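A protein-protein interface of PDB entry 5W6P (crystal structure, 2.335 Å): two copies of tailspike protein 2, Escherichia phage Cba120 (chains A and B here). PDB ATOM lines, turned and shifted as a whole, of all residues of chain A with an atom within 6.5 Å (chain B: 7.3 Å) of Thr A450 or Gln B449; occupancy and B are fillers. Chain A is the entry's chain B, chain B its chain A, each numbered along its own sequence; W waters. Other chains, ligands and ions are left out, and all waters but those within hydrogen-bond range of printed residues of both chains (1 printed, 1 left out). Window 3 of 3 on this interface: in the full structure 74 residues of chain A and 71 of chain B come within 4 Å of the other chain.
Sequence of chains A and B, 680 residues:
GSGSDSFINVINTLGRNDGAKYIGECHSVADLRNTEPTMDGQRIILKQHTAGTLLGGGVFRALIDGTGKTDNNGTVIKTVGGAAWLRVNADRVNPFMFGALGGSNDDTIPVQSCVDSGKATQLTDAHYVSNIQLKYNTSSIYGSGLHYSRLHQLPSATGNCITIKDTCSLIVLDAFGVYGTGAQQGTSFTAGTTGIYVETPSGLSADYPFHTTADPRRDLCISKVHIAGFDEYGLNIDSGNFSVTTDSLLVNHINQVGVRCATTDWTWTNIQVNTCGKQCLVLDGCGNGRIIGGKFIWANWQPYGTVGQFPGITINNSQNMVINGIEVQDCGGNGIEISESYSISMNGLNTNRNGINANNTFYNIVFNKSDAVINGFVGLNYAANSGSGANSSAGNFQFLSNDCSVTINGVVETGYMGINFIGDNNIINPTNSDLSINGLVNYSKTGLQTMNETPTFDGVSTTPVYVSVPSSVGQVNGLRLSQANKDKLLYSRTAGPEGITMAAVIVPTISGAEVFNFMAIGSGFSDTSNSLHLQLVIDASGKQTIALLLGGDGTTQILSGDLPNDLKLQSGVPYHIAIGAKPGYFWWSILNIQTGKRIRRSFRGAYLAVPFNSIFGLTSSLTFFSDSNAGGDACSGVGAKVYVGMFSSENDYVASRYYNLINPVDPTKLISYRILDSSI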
ATOM      1  N   TYR A 443      24.853  21.759   5.877  1.00  0.00           N
ATOM      2  CA  TYR A 443      23.903  21.898   4.775  1.00  0.00           C
ATOM      3  C   TYR A 443      24.594  22.305   3.481  1.00  0.00           C
ATOM      4  O   TYR A 443      24.160  21.896   2.394  1.00  0.00           O
ATOM      5  CB  TYR A 443      22.810  22.910   5.125  1.00  0.00           C
ATOM      6  CG  TYR A 443      21.810  23.147   4.003  1.00  0.00           C
ATOM      7  CD1 TYR A 443      20.745  22.278   3.789  1.00  0.00           C
ATOM      8  CD2 TYR A 443      21.930  24.245   3.162  1.00  0.00           C
ATOM      9  CE1 TYR A 443      19.830  22.499   2.767  1.00  0.00           C
ATOM     10  CE2 TYR A 443      21.020  24.471   2.138  1.00  0.00           C
ATOM     11  CZ  TYR A 443      19.976  23.595   1.945  1.00  0.00           C
ATOM     12  OH  TYR A 443      19.072  23.830   0.927  1.00  0.00           O
ATOM     13  N   LEU A 448      21.797  15.488   0.096  1.00  0.00           N
ATOM     14  CA  LEU A 448      20.703  14.663   0.583  1.00  0.00           C
ATOM     15  C   LEU A 448      19.365  15.284   0.212  1.00  0.00           C
ATOM     16  O   LEU A 448      19.161  16.493   0.347  1.00  0.00           O
ATOM     17  CB  LEU A 448      20.784  14.483   2.100  1.00  0.00           C
ATOM     18  CG  LEU A 448      21.924  13.650   2.691  1.00  0.00           C
ATOM     19  CD1 LEU A 448      22.028  13.918   4.173  1.00  0.00           C
ATOM     20  CD2 LEU A 448      21.731  12.163   2.417  1.00  0.00           C
ATOM     21  N   GLN A 449      18.446  14.441  -0.249  1.00  0.00           N
ATOM     22  CA  GLN A 449      17.088  14.854  -0.567  1.00  0.00           C
ATOM     23  C   GLN A 449      16.230  14.798   0.688  1.00  0.00           C
ATOM     24  O   GLN A 449      16.210  13.778   1.388  1.00  0.00           O
ATOM     25  CB  GLN A 449      16.498  13.940  -1.642  1.00  0.00           C
ATOM     26  CG  GLN A 449      17.242  13.962  -2.968  1.00  0.00           C
ATOM     27  CD  GLN A 449      17.260  15.347  -3.592  1.00  0.00           C
ATOM     28  OE1 GLN A 449      16.312  15.736  -4.278  1.00  0.00           O
ATOM     29  NE2 GLN A 449      18.319  16.110  -3.329  1.00  0.00           N
ATOM     30  N   THR A 450      15.507  15.879   0.959  1.00  0.00           N
ATOM     31  CA  THR A 450      14.655  15.945   2.132  1.00  0.00           C
ATOM     32  C   THR A 450      13.263  16.349   1.682  1.00  0.00           C
ATOM     33  O   THR A 450      13.075  16.858   0.577  1.00  0.00           O
ATOM     34  CB  THR A 450      15.172  16.965   3.168  1.00  0.00           C
ATOM     35  OG1 THR A 450      14.937  18.297   2.692  1.00  0.00           O
ATOM     36  CG2 THR A 450      16.668  16.793   3.397  1.00  0.00           C
ATOM     37  N   MET A 451      12.281  16.131   2.545  1.00  0.00           N
ATOM     38  CA  MET A 451      11.018  16.809   2.330  1.00  0.00           C
ATOM     39  C   MET A 451      11.237  18.317   2.426  1.00  0.00           C
ATOM     40  O   MET A 451      12.198  18.801   3.032  1.00  0.00           O
ATOM     41  CB  MET A 451       9.955  16.292   3.299  1.00  0.00           C
ATOM     42  CG  MET A 451      10.238  16.444   4.773  1.00  0.00           C
ATOM     43  SD  MET A 451       8.841  15.735   5.673  1.00  0.00           S
ATOM     44  CE  MET A 451       8.570  14.254   4.701  1.00  0.00           C
ATOM     45  N   ASN A 452      10.340  19.066   1.798  1.00  0.00           N
ATOM     46  CA  ASN A 452      10.386  20.521   1.907  1.00  0.00           C
ATOM     47  C   ASN A 452       8.951  21.023   1.759  1.00  0.00           C
ATOM     48  O   ASN A 452       8.504  21.356   0.659  1.00  0.00           O
ATOM     49  CB  ASN A 452      11.313  21.133   0.868  1.00  0.00           C
ATOM     50  CG  ASN A 452      11.632  22.582   1.159  1.00  0.00           C
ATOM     51  OD1 ASN A 452      10.824  23.294   1.758  1.00  0.00           O
ATOM     52  ND2 ASN A 452      12.816  23.028   0.748  1.00  0.00           N
ATOM     53  N   PRO A 667      20.166  18.977   8.440  1.00  0.00           N
ATOM     54  CA  PRO A 667      19.590  18.351   7.240  1.00  0.00           C
ATOM     55  C   PRO A 667      18.823  17.062   7.511  1.00  0.00           C
ATOM     56  O   PRO A 667      17.839  16.785   6.809  1.00  0.00           O
ATOM     57  CB  PRO A 667      20.825  18.094   6.368  1.00  0.00           C
ATOM     58  CG  PRO A 667      21.779  19.151   6.766  1.00  0.00           C
ATOM     59  CD  PRO A 667      21.587  19.320   8.253  1.00  0.00           C
ATOM     60  N   THR A 668      19.231  16.261   8.499  1.00  0.00           N
ATOM     61  CA  THR A 668      18.507  15.020   8.759  1.00  0.00           C
ATOM     62  C   THR A 668      17.168  15.267   9.439  1.00  0.00           C
ATOM     63  O   THR A 668      16.335  14.355   9.486  1.00  0.00           O
ATOM     64  CB  THR A 668      19.349  14.051   9.602  1.00  0.00           C
ATOM     65  OG1 THR A 668      19.469  14.540  10.938  1.00  0.00           O
ATOM     66  CG2 THR A 668      20.744  13.920   9.018  1.00  0.00           C
ATOM     67  N   LEU A 670      15.420  18.265   8.589  1.00  0.00           N
ATOM     68  CA  LEU A 670      14.847  19.368   7.829  1.00  0.00           C
ATOM     69  C   LEU A 670      13.468  18.995   7.293  1.00  0.00           C
ATOM     70  O   LEU A 670      13.297  17.949   6.661  1.00  0.00           O
ATOM     71  CB  LEU A 670      15.795  19.749   6.695  1.00  0.00           C
ATOM     72  CG  LEU A 670      15.539  21.037   5.924  1.00  0.00           C
ATOM     73  CD1 LEU A 670      16.840  21.526   5.307  1.00  0.00           C
ATOM     74  CD2 LEU A 670      14.485  20.804   4.845  1.00  0.00           C
ATOM     75  N   ILE A 671      12.481  19.852   7.563  1.00  0.00           N
ATOM     76  CA  ILE A 671      11.114  19.659   7.100  1.00  0.00           C
ATOM     77  C   ILE A 671      10.747  20.639   5.989  1.00  0.00           C
ATOM     78  O   ILE A 671      10.052  20.277   5.034  1.00  0.00           O
ATOM     79  CB  ILE A 671      10.128  19.791   8.283  1.00  0.00           C
ATOM     80  CG1 ILE A 671      10.397  18.722   9.344  1.00  0.00           C
ATOM     81  CG2 ILE A 671       8.687  19.758   7.789  1.00  0.00           C
ATOM     82  CD1 ILE A 671      10.459  17.320   8.790  1.00  0.00           C
ATOM     83  N   SER A 672      11.208  21.882   6.102  1.00  0.00           N
ATOM     84  CA  SER A 672      10.945  22.918   5.119  1.00  0.00           C
ATOM     85  C   SER A 672      12.111  23.890   5.140  1.00  0.00           C
ATOM     86  O   SER A 672      12.658  24.192   6.203  1.00  0.00           O
ATOM     87  CB  SER A 672       9.633  23.655   5.424  1.00  0.00           C
ATOM     88  OG  SER A 672       9.307  24.581   4.401  1.00  0.00           O
ATOM     89  N   THR B 446      12.904  12.693  11.278  1.00  0.00           N
ATOM     90  CA  THR B 446      13.646  12.927  10.049  1.00  0.00           C
ATOM     91  C   THR B 446      12.724  13.271   8.882  1.00  0.00           C
ATOM     92  O   THR B 446      11.600  12.768   8.778  1.00  0.00           O
ATOM     93  CB  THR B 446      14.506  11.715   9.685  1.00  0.00           C
ATOM     94  OG1 THR B 446      15.402  12.072   8.626  1.00  0.00           O
ATOM     95  CG2 THR B 446      13.630  10.549   9.244  1.00  0.00           C
ATOM     96  N   GLY B 447      13.230  14.122   7.989  1.00  0.00           N
ATOM     97  CA  GLY B 447      12.583  14.373   6.717  1.00  0.00           C
ATOM     98  C   GLY B 447      13.368  13.777   5.561  1.00  0.00           C
ATOM     99  O   GLY B 447      13.139  14.127   4.399  1.00  0.00           O
ATOM    100  N   LEU B 448      14.292  12.867   5.866  1.00  0.00           N
ATOM    101  CA  LEU B 448      15.148  12.297   4.836  1.00  0.00           C
ATOM    102  C   LEU B 448      14.334  11.445   3.871  1.00  0.00           C
ATOM    103  O   LEU B 448      13.467  10.664   4.274  1.00  0.00           O
ATOM    104  CB  LEU B 448      16.259  11.453   5.462  1.00  0.00           C
ATOM    105  CG  LEU B 448      17.325  12.222   6.252  1.00  0.00           C
ATOM    106  CD1 LEU B 448      18.123  11.272   7.132  1.00  0.00           C
ATOM    107  CD2 LEU B 448      18.238  13.007   5.333  1.00  0.00           C
ATOM    108  N   GLN B 449      14.606  11.613   2.584  1.00  0.00           N
ATOM    109  CA  GLN B 449      13.978  10.798   1.562  1.00  0.00           C
ATOM    110  C   GLN B 449      14.826   9.556   1.320  1.00  0.00           C
ATOM    111  O   GLN B 449      16.046   9.656   1.144  1.00  0.00           O
ATOM    112  CB  GLN B 449      13.799  11.594   0.272  1.00  0.00           C
ATOM    113  CG  GLN B 449      12.959  12.852   0.465  1.00  0.00           C
ATOM    114  CD  GLN B 449      11.592  12.558   1.067  1.00  0.00           C
ATOM    115  OE1 GLN B 449      10.656  12.176   0.359  1.00  0.00           O
ATOM    116  NE2 GLN B 449      11.468  12.745   2.378  1.00  0.00           N
ATOM    117  N   THR B 450      14.180   8.392   1.325  1.00  0.00           N
ATOM    118  CA  THR B 450      14.847   7.118   1.130  1.00  0.00           C
ATOM    119  C   THR B 450      14.110   6.329   0.058  1.00  0.00           C
ATOM    120  O   THR B 450      13.019   6.701  -0.375  1.00  0.00           O
ATOM    121  CB  THR B 450      14.898   6.296   2.428  1.00  0.00           C
ATOM    122  OG1 THR B 450      13.593   5.779   2.730  1.00  0.00           O
ATOM    123  CG2 THR B 450      15.372   7.158   3.584  1.00  0.00           C
ATOM    124  N   MET B 451      14.726   5.231  -0.370  1.00  0.00           N
ATOM    125  CA  MET B 451      13.979   4.218  -1.097  1.00  0.00           C
ATOM    126  C   MET B 451      12.813   3.736  -0.245  1.00  0.00           C
ATOM    127  O   MET B 451      12.866   3.749   0.987  1.00  0.00           O
ATOM    128  CB  MET B 451      14.856   3.009  -1.421  1.00  0.00           C
ATOM    129  CG  MET B 451      16.162   3.285  -2.106  1.00  0.00           C
ATOM    130  SD  MET B 451      17.038   1.712  -2.269  1.00  0.00           S
ATOM    131  CE  MET B 451      15.709   0.632  -2.789  1.00  0.00           C
ATOM    132  N   PRO B 667      17.082   4.880   9.518  1.00  0.00           N
ATOM    133  CA  PRO B 667      16.715   5.631   8.307  1.00  0.00           C
ATOM    134  C   PRO B 667      17.784   5.645   7.222  1.00  0.00           C
ATOM    135  O   PRO B 667      17.429   5.668   6.033  1.00  0.00           O
ATOM    136  CB  PRO B 667      16.433   7.036   8.853  1.00  0.00           C
ATOM    137  CG  PRO B 667      15.943   6.789  10.234  1.00  0.00           C
ATOM    138  CD  PRO B 667      16.770   5.629  10.747  1.00  0.00           C
HETATM  139  O   HOH W   1      18.299  11.577   2.017  1.00  0.00           O
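The backbone NH of Leu B448 lies close to the side-chain hydroxyl of Thr B446, at 3.1 Å.
The side-chain amide nitrogen (NE2) of Gln B449 sits at hydrogen-bond distance from the backbone carbonyl oxygen (O) of Gly B447, at 3.0 Å.
Water W1 bridges the backbone carbonyl oxygen of Gln B449 and the backbone carbonyl oxygen of Gln A449.
The side-chain hydroxyl (OG1) of Thr B446 lies within hydrogen-bond range of the backbone carbonyl oxygen (O) of Thr A668 (2.6 Å).
O of Gly B447 sits at hydrogen-bond distance from N of Met A451, at 2.9 Å.
The backbone NH of Gly B447 is in hydrogen-bond range of the backbone carbonyl oxygen of Thr A668 (3.5 Å).
The backbone carbonyl oxygen (O) of Gln A449 is in hydrogen-bond range of the backbone NH (N) of Gln B449, 2.9 Å away.
The side-chain amide nitrogen of Gln B449 lies close to the backbone NH of Met A451 (3.5 Å).
Gln A449 touches Leu B448, but with the chains exchanged Leu A448 does not touch Gln B449 (6.3 Å).
Gln B449 touches its own counterpart, Gln A449.
Thr A450 touches Gln B449, but with the chains exchanged Gln A449 does not touch Thr B450 (5.8 Å).
Met A451 touches Gln B449, but with the chains exchanged Gln A449 does not touch Met B451 (8.9 Å).
Positions printed for both chains: 448, 449, 450, 451 and 667.
Among the printed residues, pairs that only touch across the chains: Gln A449 with Leu B448 (3.9 Å), Thr A450 with Gly B447 (3.3 Å), Thr A450 with Gln B449 (3.7 Å), Thr A668 with Leu B448 (3.9 Å) and Leu A670 with Gly B447 (3.6 Å).
Of the 11 printed residues of chain A, 5 touch a printed residue of chain B.
Printed residues of chain A that touch a printed residue of chain B: Gln A449, Thr A450, Met A451, Thr A668 and Leu A670.
Of the 7 printed residues of chain B, 4 touch a printed residue of chain A.
Printed residues of chain B that touch a printed residue of chain A: Thr B446, Gly B447, Leu B448 and Gln B449.
Hydrophobic or aromatic side chains of chain B within 4 Å of the printed part of chain A: Leu B448.
Among the printed residues, 10 pairs touch across the chains.
Of chain B, only Gly B447 and Gln B449 come within 4 Å of Thr A450.
Printed residues of chain A within 4 Å of Leu B448: Gln A449 and Thr A668.
Of the printed residues of chain B, Gln A449 touches Leu B448 (3.9 Å) and Gln B449 (2.9 Å).
The nearest residue of chain A that does not touch Gln B449 is Leu A448 (6.3 Å).
The nearest printed residue of chain B that does not touch Leu A670 is Thr B446 (5.2 Å).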
